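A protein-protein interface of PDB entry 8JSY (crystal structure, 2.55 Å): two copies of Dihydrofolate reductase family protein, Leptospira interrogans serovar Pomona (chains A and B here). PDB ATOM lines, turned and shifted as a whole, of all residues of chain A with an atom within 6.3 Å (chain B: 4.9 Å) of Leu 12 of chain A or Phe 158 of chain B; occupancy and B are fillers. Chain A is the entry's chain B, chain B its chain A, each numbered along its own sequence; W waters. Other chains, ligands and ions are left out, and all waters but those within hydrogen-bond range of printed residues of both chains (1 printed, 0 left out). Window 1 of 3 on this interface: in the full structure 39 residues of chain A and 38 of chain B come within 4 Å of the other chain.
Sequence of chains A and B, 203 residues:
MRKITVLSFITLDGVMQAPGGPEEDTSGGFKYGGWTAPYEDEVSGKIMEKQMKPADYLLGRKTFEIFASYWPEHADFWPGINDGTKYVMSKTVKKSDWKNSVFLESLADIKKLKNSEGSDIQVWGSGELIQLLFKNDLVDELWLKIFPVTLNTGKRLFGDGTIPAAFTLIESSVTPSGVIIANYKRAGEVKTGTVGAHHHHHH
O of Pro 148 of chain A sits at hydrogen-bond distance from N of Phe 167 of chain B, 2.7 Å away.
ND2 of Asn 152 of chain A lies close to O of Thr 162 of chain B, 3.0 Å away.
NH1 of Arg 156 of chain B sits close to NH1 of Arg 156 of chain A, at 3.5 Å.
The backbone carbonyl oxygen (O) of Leu 142 of chain B lies within hydrogen-bond range of the backbone NH (N) of Tyr 184 of chain B (2.8 Å).
O of Phe 147 of chain A sits at hydrogen-bond distance from N of Leu 12 of chain A (3.3 Å).
The backbone carbonyl oxygen (O) of Gly 159 of chain B lies within hydrogen-bond range of the side-chain hydroxyl (OG1) of Thr 162 of chain B.
The backbone NH of Leu 12 of chain A lies within hydrogen-bond range of the backbone carbonyl oxygen of Val 149 of chain A, at 2.9 Å.
The side-chain carboxylate (OD1) of Asp 13 of chain A sits at hydrogen-bond distance from the side-chain hydroxyl (OG1) of Thr 150 of chain A (3.3 Å).
OD1 of Asp 13 of chain A sits at hydrogen-bond distance from OG1 of Thr 11 of chain A (2.7 Å).
CD1 of Leu 144 of chain B touches CD2 of Leu 12 of chain A, at 3.99 Å.
CE2 of Phe 158 of chain B touches O of Leu 12 of chain A, 3.6 Å away.
Leu 12 of chain A touches Tyr 184 of chain B (CD2 to OH, 3.5 Å).
Asp 13 of chain A touches Arg 156 of chain B.
Phe 158 of chain B touches Asp 13 of chain A.
CB of Pro 148 of chain A touches CE1 of Tyr 184 of chain B (3.9 Å).
Thr 162 of chain B touches Thr 150 of chain A.
CG2 of Thr 150 of chain A touches CE1 of Phe 167 of chain B (3.7 Å).
Tyr 184 of chain B touches Ile 180 of chain A (OH to CD1, 3.1 Å).
Printed residues of chain B within 4 Å of Leu 12 of chain A: Leu 144, Phe 158 and Tyr 184.
Printed residues of chain B within 4 Å of Ile 180 of chain A: Tyr 184 (3.1 Å).
Leu 157 of chain B touches none of the printed residues of chain A.
Phe 158 of chain B touches just these residues of chain A: Leu 12 (3.6 Å) and Asp 13 (3.5 Å).
Asp 160 of chain B touches none of the printed residues of chain A.
Printed residues of chain A within 4 Å of Phe 167 of chain B: Pro 148 and Thr 150.
The nearest residue of chain A that does not touch Phe 158 of chain B is Thr 150 of chain A (4.1 Å).
The nearest printed residue of chain B that does not touch Pro 148 of chain A is Leu 144 of chain B (8.6 Å).
Hydrophobic or aromatic side chains of chain B that line the printed part of chain A: Leu 144, Phe 158, Phe 167 and Tyr 184.
Of the 14 printed residues of chain A, 7 touch a printed residue of chain B.
Hydrophobic or aromatic side chains of chain A within 4 Å of the printed part of chain B: Leu 12, Pro 148 and Ile 180.
Among the printed residues, no Asp or Glu carboxylate lies within 4 Å of a Lys or Arg side-chain nitrogen of the other chain.
Arg 156 of chain B touches its own counterpart, Arg 156 of chain A.
Positions printed for both chains: 14 and 156.
Water W1 bridges the backbone carbonyl oxygen (O) of Leu 12 of chain A (3.3 Å) and the backbone NH (N) of Gly 14 of chain B (3.5 Å).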
ATOM      1  N   ILE A  10       7.477   1.922   1.572  1.00  0.00           N
ATOM      2  CA  ILE A  10       7.050   3.090   2.330  1.00  0.00           C
ATOM      3  C   ILE A  10       5.586   3.347   2.060  1.00  0.00           C
ATOM      4  O   ILE A  10       5.063   3.018   0.990  1.00  0.00           O
ATOM      5  CB  ILE A  10       7.874   4.349   1.985  1.00  0.00           C
ATOM      6  CG1 ILE A  10       8.152   4.415   0.486  1.00  0.00           C
ATOM      7  CG2 ILE A  10       9.196   4.369   2.749  1.00  0.00           C
ATOM      8  CD1 ILE A  10       8.547   5.805   0.029  1.00  0.00           C
ATOM      9  N   THR A  11       4.927   3.942   3.048  1.00  0.00           N
ATOM     10  CA  THR A  11       3.555   4.399   2.912  1.00  0.00           C
ATOM     11  C   THR A  11       3.510   5.695   2.107  1.00  0.00           C
ATOM     12  O   THR A  11       4.538   6.262   1.713  1.00  0.00           O
ATOM     13  CB  THR A  11       2.929   4.626   4.285  1.00  0.00           C
ATOM     14  OG1 THR A  11       3.694   5.611   4.993  1.00  0.00           O
ATOM     15  CG2 THR A  11       2.918   3.342   5.086  1.00  0.00           C
ATOM     16  N   LEU A  12       2.288   6.185   1.884  1.00  0.00           N
ATOM     17  CA  LEU A  12       2.125   7.495   1.266  1.00  0.00           C
ATOM     18  C   LEU A  12       2.818   8.560   2.094  1.00  0.00           C
ATOM     19  O   LEU A  12       3.466   9.462   1.550  1.00  0.00           O
ATOM     20  CB  LEU A  12       0.643   7.826   1.103  1.00  0.00           C
ATOM     21  CG  LEU A  12       0.019   7.496  -0.252  1.00  0.00           C
ATOM     22  CD1 LEU A  12      -1.441   7.915  -0.271  1.00  0.00           C
ATOM     23  CD2 LEU A  12       0.805   8.167  -1.377  1.00  0.00           C
ATOM     24  N   ASP A  13       2.724   8.464   3.416  1.00  0.00           N
ATOM     25  CA  ASP A  13       3.402   9.429   4.255  1.00  0.00           C
ATOM     26  C   ASP A  13       4.781   8.960   4.692  1.00  0.00           C
ATOM     27  O   ASP A  13       5.353   9.539   5.627  1.00  0.00           O
ATOM     28  CB  ASP A  13       2.521   9.800   5.443  1.00  0.00           C
ATOM     29  CG  ASP A  13       2.342   8.678   6.423  1.00  0.00           C
ATOM     30  OD1 ASP A  13       2.098   7.521   6.001  1.00  0.00           O
ATOM     31  OD2 ASP A  13       2.407   8.990   7.632  1.00  0.00           O
ATOM     32  N   GLY A  14       5.327   7.943   4.019  1.00  0.00           N
ATOM     33  CA  GLY A  14       6.714   7.565   4.207  1.00  0.00           C
ATOM     34  C   GLY A  14       7.055   6.773   5.452  1.00  0.00           C
ATOM     35  O   GLY A  14       8.174   6.896   5.963  1.00  0.00           O
ATOM     36  N   VAL A  15       6.139   5.958   5.967  1.00  0.00           N
ATOM     37  CA  VAL A  15       6.469   5.082   7.085  1.00  0.00           C
ATOM     38  C   VAL A  15       7.091   3.808   6.532  1.00  0.00           C
ATOM     39  O   VAL A  15       6.553   3.176   5.612  1.00  0.00           O
ATOM     40  CB  VAL A  15       5.240   4.775   7.956  1.00  0.00           C
ATOM     41  CG1 VAL A  15       5.422   3.444   8.688  1.00  0.00           C
ATOM     42  CG2 VAL A  15       5.021   5.882   8.978  1.00  0.00           C
ATOM     43  N   ILE A 146       5.817   2.505  -3.016  1.00  0.00           N
ATOM     44  CA  ILE A 146       4.929   3.413  -2.301  1.00  0.00           C
ATOM     45  C   ILE A 146       3.545   2.798  -2.253  1.00  0.00           C
ATOM     46  O   ILE A 146       2.971   2.454  -3.298  1.00  0.00           O
ATOM     47  CB  ILE A 146       4.900   4.792  -2.968  1.00  0.00           C
ATOM     48  CG1 ILE A 146       6.333   5.318  -3.069  1.00  0.00           C
ATOM     49  CG2 ILE A 146       3.989   5.735  -2.183  1.00  0.00           C
ATOM     50  CD1 ILE A 146       6.537   6.392  -4.089  1.00  0.00           C
ATOM     51  N   PHE A 147       3.004   2.673  -1.036  1.00  0.00           N
ATOM     52  CA  PHE A 147       1.794   1.912  -0.828  1.00  0.00           C
ATOM     53  C   PHE A 147       0.603   2.820  -0.529  1.00  0.00           C
ATOM     54  O   PHE A 147       0.740   3.812   0.201  1.00  0.00           O
ATOM     55  CB  PHE A 147       2.001   0.901   0.312  1.00  0.00           C
ATOM     56  CG  PHE A 147       2.920  -0.254  -0.058  1.00  0.00           C
ATOM     57  CD1 PHE A 147       4.299  -0.062  -0.163  1.00  0.00           C
ATOM     58  CD2 PHE A 147       2.401  -1.520  -0.320  1.00  0.00           C
ATOM     59  CE1 PHE A 147       5.140  -1.113  -0.515  1.00  0.00           C
ATOM     60  CE2 PHE A 147       3.239  -2.577  -0.677  1.00  0.00           C
ATOM     61  CZ  PHE A 147       4.607  -2.375  -0.770  1.00  0.00           C
ATOM     62  N   PRO A 148      -0.581   2.488  -1.069  1.00  0.00           N
ATOM     63  CA  PRO A 148      -1.729   3.400  -0.982  1.00  0.00           C
ATOM     64  C   PRO A 148      -2.336   3.425   0.402  1.00  0.00           C
ATOM     65  O   PRO A 148      -3.530   3.158   0.587  1.00  0.00           O
ATOM     66  CB  PRO A 148      -2.707   2.820  -2.007  1.00  0.00           C
ATOM     67  CG  PRO A 148      -2.435   1.358  -1.962  1.00  0.00           C
ATOM     68  CD  PRO A 148      -0.947   1.206  -1.699  1.00  0.00           C
ATOM     69  N   VAL A 149      -1.509   3.739   1.394  1.00  0.00           N
ATOM     70  CA  VAL A 149      -1.954   3.707   2.775  1.00  0.00           C
ATOM     71  C   VAL A 149      -1.249   4.818   3.533  1.00  0.00           C
ATOM     72  O   VAL A 149      -0.166   5.281   3.158  1.00  0.00           O
ATOM     73  CB  VAL A 149      -1.684   2.331   3.436  1.00  0.00           C
ATOM     74  CG1 VAL A 149      -0.255   2.248   4.018  1.00  0.00           C
ATOM     75  CG2 VAL A 149      -2.723   2.056   4.464  1.00  0.00           C
ATOM     76  N   THR A 150      -1.872   5.245   4.621  1.00  0.00           N
ATOM     77  CA  THR A 150      -1.270   6.244   5.476  1.00  0.00           C
ATOM     78  C   THR A 150      -1.393   5.780   6.927  1.00  0.00           C
ATOM     79  O   THR A 150      -2.421   5.215   7.323  1.00  0.00           O
ATOM     80  CB  THR A 150      -1.920   7.611   5.179  1.00  0.00           C
ATOM     81  OG1 THR A 150      -1.006   8.662   5.501  1.00  0.00           O
ATOM     82  CG2 THR A 150      -3.250   7.807   5.876  1.00  0.00           C
ATOM     83  N   ASN A 152      -0.032   7.091  11.007  1.00  0.00           N
ATOM     84  CA  ASN A 152       0.526   8.321  11.552  1.00  0.00           C
ATOM     85  C   ASN A 152       1.949   8.113  12.057  1.00  0.00           C
ATOM     86  O   ASN A 152       2.896   8.721  11.551  1.00  0.00           O
ATOM     87  CB  ASN A 152      -0.372   8.862  12.655  1.00  0.00           C
ATOM     88  CG  ASN A 152      -0.190  10.337  12.848  1.00  0.00           C
ATOM     89  OD1 ASN A 152       0.468  10.995  12.024  1.00  0.00           O
ATOM     90  ND2 ASN A 152      -0.792  10.887  13.916  1.00  0.00           N
ATOM     91  N   ARG A 156      10.506   6.279   9.932  1.00  0.00           N
ATOM     92  CA  ARG A 156      10.381   6.861   8.598  1.00  0.00           C
ATOM     93  C   ARG A 156      11.654   6.624   7.808  1.00  0.00           C
ATOM     94  O   ARG A 156      12.750   6.640   8.369  1.00  0.00           O
ATOM     95  CB  ARG A 156      10.097   8.366   8.678  1.00  0.00           C
ATOM     96  CG  ARG A 156       8.986   8.747   9.657  1.00  0.00           C
ATOM     97  CD  ARG A 156       8.653  10.220   9.587  1.00  0.00           C
ATOM     98  NE  ARG A 156       8.948  10.754   8.264  1.00  0.00           N
ATOM     99  CZ  ARG A 156       8.095  10.767   7.245  1.00  0.00           C
ATOM    100  NH1 ARG A 156       8.466  11.180   6.034  1.00  0.00           N
ATOM    101  NH2 ARG A 156       6.841  10.358   7.444  1.00  0.00           N
ATOM    102  N   ILE A 180       3.262   1.876  -6.196  1.00  0.00           N
ATOM    103  CA  ILE A 180       4.045   2.602  -7.186  1.00  0.00           C
ATOM    104  C   ILE A 180       5.510   2.239  -7.009  1.00  0.00           C
ATOM    105  O   ILE A 180       6.085   2.419  -5.926  1.00  0.00           O
ATOM    106  CB  ILE A 180       3.811   4.117  -7.093  1.00  0.00           C
ATOM    107  CG1 ILE A 180       2.371   4.429  -7.497  1.00  0.00           C
ATOM    108  CG2 ILE A 180       4.794   4.885  -7.973  1.00  0.00           C
ATOM    109  CD1 ILE A 180       1.887   5.706  -6.968  1.00  0.00           C
ATOM    110  N   GLY B  14       7.777  14.242   1.454  1.00  0.00           N
ATOM    111  CA  GLY B  14       6.521  14.834   1.895  1.00  0.00           C
ATOM    112  C   GLY B  14       6.520  16.301   2.292  1.00  0.00           C
ATOM    113  O   GLY B  14       5.672  16.712   3.087  1.00  0.00           O
ATOM    114  N   GLN B 131      -4.407  19.531   7.755  1.00  0.00           N
ATOM    115  CA  GLN B 131      -4.282  18.749   8.982  1.00  0.00           C
ATOM    116  C   GLN B 131      -5.639  18.600   9.665  1.00  0.00           C
ATOM    117  O   GLN B 131      -6.010  17.499  10.109  1.00  0.00           O
ATOM    118  CB  GLN B 131      -3.262  19.396   9.923  1.00  0.00           C
ATOM    119  CG  GLN B 131      -1.813  19.305   9.428  1.00  0.00           C
ATOM    120  CD  GLN B 131      -1.585  18.126   8.506  1.00  0.00           C
ATOM    121  OE1 GLN B 131      -1.530  16.972   8.945  1.00  0.00           O
ATOM    122  NE2 GLN B 131      -1.453  18.403   7.223  1.00  0.00           N
ATOM    123  N   PHE B 134      -7.812  16.147   7.493  1.00  0.00           N
ATOM    124  CA  PHE B 134      -7.336  14.774   7.639  1.00  0.00           C
ATOM    125  C   PHE B 134      -7.784  14.169   8.964  1.00  0.00           C
ATOM    126  O   PHE B 134      -8.251  13.022   9.010  1.00  0.00           O
ATOM    127  CB  PHE B 134      -5.808  14.750   7.557  1.00  0.00           C
ATOM    128  CG  PHE B 134      -5.270  14.657   6.163  1.00  0.00           C
ATOM    129  CD1 PHE B 134      -6.075  14.204   5.129  1.00  0.00           C
ATOM    130  CD2 PHE B 134      -3.944  14.999   5.894  1.00  0.00           C
ATOM    131  CE1 PHE B 134      -5.569  14.101   3.840  1.00  0.00           C
ATOM    132  CE2 PHE B 134      -3.433  14.898   4.617  1.00  0.00           C
ATOM    133  CZ  PHE B 134      -4.251  14.445   3.581  1.00  0.00           C
ATOM    134  N   LEU B 142      -7.267  12.398  -3.265  1.00  0.00           N
ATOM    135  CA  LEU B 142      -5.937  13.005  -3.232  1.00  0.00           C
ATOM    136  C   LEU B 142      -5.351  13.041  -4.633  1.00  0.00           C
ATOM    137  O   LEU B 142      -5.252  12.002  -5.286  1.00  0.00           O
ATOM    138  CB  LEU B 142      -4.979  12.224  -2.320  1.00  0.00           C
ATOM    139  CG  LEU B 142      -5.065  12.316  -0.799  1.00  0.00           C
ATOM    140  CD1 LEU B 142      -3.687  12.103  -0.173  1.00  0.00           C
ATOM    141  CD2 LEU B 142      -5.587  13.658  -0.420  1.00  0.00           C
ATOM    142  N   LEU B 144      -1.865  13.978  -6.124  1.00  0.00           N
ATOM    143  CA  LEU B 144      -0.517  14.288  -5.700  1.00  0.00           C
ATOM    144  C   LEU B 144       0.399  14.367  -6.905  1.00  0.00           C
ATOM    145  O   LEU B 144       0.207  13.665  -7.906  1.00  0.00           O
ATOM    146  CB  LEU B 144       0.002  13.224  -4.726  1.00  0.00           C
ATOM    147  CG  LEU B 144      -0.851  12.986  -3.479  1.00  0.00           C
ATOM    148  CD1 LEU B 144      -0.475  11.667  -2.795  1.00  0.00           C
ATOM    149  CD2 LEU B 144      -0.712  14.163  -2.508  1.00  0.00           C
ATOM    150  N   ARG B 156       4.741  20.062   5.965  1.00  0.00           N
ATOM    151  CA  ARG B 156       4.517  18.739   5.414  1.00  0.00           C
ATOM    152  C   ARG B 156       3.042  18.533   5.100  1.00  0.00           C
ATOM    153  O   ARG B 156       2.168  19.039   5.806  1.00  0.00           O
ATOM    154  CB  ARG B 156       5.027  17.677   6.388  1.00  0.00           C
ATOM    155  CG  ARG B 156       6.533  17.741   6.611  1.00  0.00           C
ATOM    156  CD  ARG B 156       7.040  16.526   7.361  1.00  0.00           C
ATOM    157  NE  ARG B 156       6.139  15.394   7.185  1.00  0.00           N
ATOM    158  CZ  ARG B 156       6.323  14.443   6.276  1.00  0.00           C
ATOM    159  NH1 ARG B 156       7.395  14.435   5.499  1.00  0.00           N
ATOM    160  NH2 ARG B 156       5.408  13.476   6.143  1.00  0.00           N
ATOM    161  N   LEU B 157       2.769  17.813   4.012  1.00  0.00           N
ATOM    162  CA  LEU B 157       1.386  17.503   3.679  1.00  0.00           C
ATOM    163  C   LEU B 157       0.779  16.517   4.675  1.00  0.00           C
ATOM    164  O   LEU B 157      -0.369  16.683   5.100  1.00  0.00           O
ATOM    165  CB  LEU B 157       1.314  16.954   2.261  1.00  0.00           C
ATOM    166  CG  LEU B 157      -0.007  16.263   1.988  1.00  0.00           C
ATOM    167  CD1 LEU B 157      -1.139  17.286   2.011  1.00  0.00           C
ATOM    168  CD2 LEU B 157       0.049  15.518   0.683  1.00  0.00           C
ATOM    169  N   PHE B 158       1.524  15.478   5.053  1.00  0.00           N
ATOM    170  CA  PHE B 158       1.085  14.514   6.073  1.00  0.00           C
ATOM    171  C   PHE B 158       1.760  14.910   7.379  1.00  0.00           C
ATOM    172  O   PHE B 158       2.888  14.487   7.675  1.00  0.00           O
ATOM    173  CB  PHE B 158       1.425  13.088   5.676  1.00  0.00           C
ATOM    174  CG  PHE B 158       0.752  12.640   4.415  1.00  0.00           C
ATOM    175  CD1 PHE B 158      -0.628  12.533   4.353  1.00  0.00           C
ATOM    176  CD2 PHE B 158       1.501  12.341   3.284  1.00  0.00           C
ATOM    177  CE1 PHE B 158      -1.245  12.128   3.195  1.00  0.00           C
ATOM    178  CE2 PHE B 158       0.886  11.913   2.109  1.00  0.00           C
ATOM    179  CZ  PHE B 158      -0.485  11.811   2.061  1.00  0.00           C
ATOM    180  N   GLY B 159       1.053  15.742   8.155  1.00  0.00           N
ATOM    181  CA  GLY B 159       1.570  16.261   9.399  1.00  0.00           C
ATOM    182  C   GLY B 159       0.720  15.888  10.594  1.00  0.00           C
ATOM    183  O   GLY B 159       0.217  14.763  10.681  1.00  0.00           O
ATOM    184  N   ASP B 160       0.516  16.860  11.488  1.00  0.00           N
ATOM    185  CA  ASP B 160      -0.135  16.617  12.770  1.00  0.00           C
ATOM    186  C   ASP B 160      -1.441  15.844  12.642  1.00  0.00           C
ATOM    187  O   ASP B 160      -1.770  15.024  13.509  1.00  0.00           O
ATOM    188  CB  ASP B 160      -0.410  17.952  13.453  1.00  0.00           C
ATOM    189  CG  ASP B 160       0.633  18.298  14.467  1.00  0.00           C
ATOM    190  OD1 ASP B 160       0.515  19.379  15.087  1.00  0.00           O
ATOM    191  OD2 ASP B 160       1.577  17.492  14.639  1.00  0.00           O
ATOM    192  N   THR B 162      -2.625  13.694  10.268  1.00  0.00           N
ATOM    193  CA  THR B 162      -2.690  12.410   9.582  1.00  0.00           C
ATOM    194  C   THR B 162      -3.199  11.306  10.503  1.00  0.00           C
ATOM    195  O   THR B 162      -2.779  11.187  11.663  1.00  0.00           O
ATOM    196  CB  THR B 162      -1.314  12.028   9.059  1.00  0.00           C
ATOM    197  OG1 THR B 162      -0.593  13.223   8.737  1.00  0.00           O
ATOM    198  CG2 THR B 162      -1.451  11.109   7.843  1.00  0.00           C
ATOM    199  N   PHE B 167      -6.151   3.734   0.950  1.00  0.00           N
ATOM    200  CA  PHE B 167      -6.520   4.423  -0.283  1.00  0.00           C
ATOM    201  C   PHE B 167      -6.429   3.464  -1.464  1.00  0.00           C
ATOM    202  O   PHE B 167      -5.791   2.412  -1.395  1.00  0.00           O
ATOM    203  CB  PHE B 167      -5.625   5.655  -0.558  1.00  0.00           C
ATOM    204  CG  PHE B 167      -5.693   6.728   0.515  1.00  0.00           C
ATOM    205  CD1 PHE B 167      -4.890   6.656   1.650  1.00  0.00           C
ATOM    206  CD2 PHE B 167      -6.552   7.807   0.385  1.00  0.00           C
ATOM    207  CE1 PHE B 167      -4.952   7.630   2.634  1.00  0.00           C
ATOM    208  CE2 PHE B 167      -6.617   8.781   1.362  1.00  0.00           C
ATOM    209  CZ  PHE B 167      -5.818   8.692   2.486  1.00  0.00           C
ATOM    210  N   TYR B 184      -5.399   9.229  -5.709  1.00  0.00           N
ATOM    211  CA  TYR B 184      -5.950   8.221  -4.812  1.00  0.00           C
ATOM    212  C   TYR B 184      -7.371   8.562  -4.368  1.00  0.00           C
ATOM    213  O   TYR B 184      -7.789   9.724  -4.363  1.00  0.00           O
ATOM    214  CB  TYR B 184      -5.085   8.057  -3.560  1.00  0.00           C
ATOM    215  CG  TYR B 184      -3.656   7.695  -3.821  1.00  0.00           C
ATOM    216  CD1 TYR B 184      -3.247   6.369  -3.845  1.00  0.00           C
ATOM    217  CD2 TYR B 184      -2.704   8.681  -4.035  1.00  0.00           C
ATOM    218  CE1 TYR B 184      -1.920   6.030  -4.076  1.00  0.00           C
ATOM    219  CE2 TYR B 184      -1.379   8.358  -4.267  1.00  0.00           C
ATOM    220  CZ  TYR B 184      -0.989   7.030  -4.287  1.00  0.00           C
ATOM    221  OH  TYR B 184       0.336   6.708  -4.521  1.00  0.00           O
HETATM  222  O   HOH W   1       5.833  11.593   2.576  1.00  0.00           O
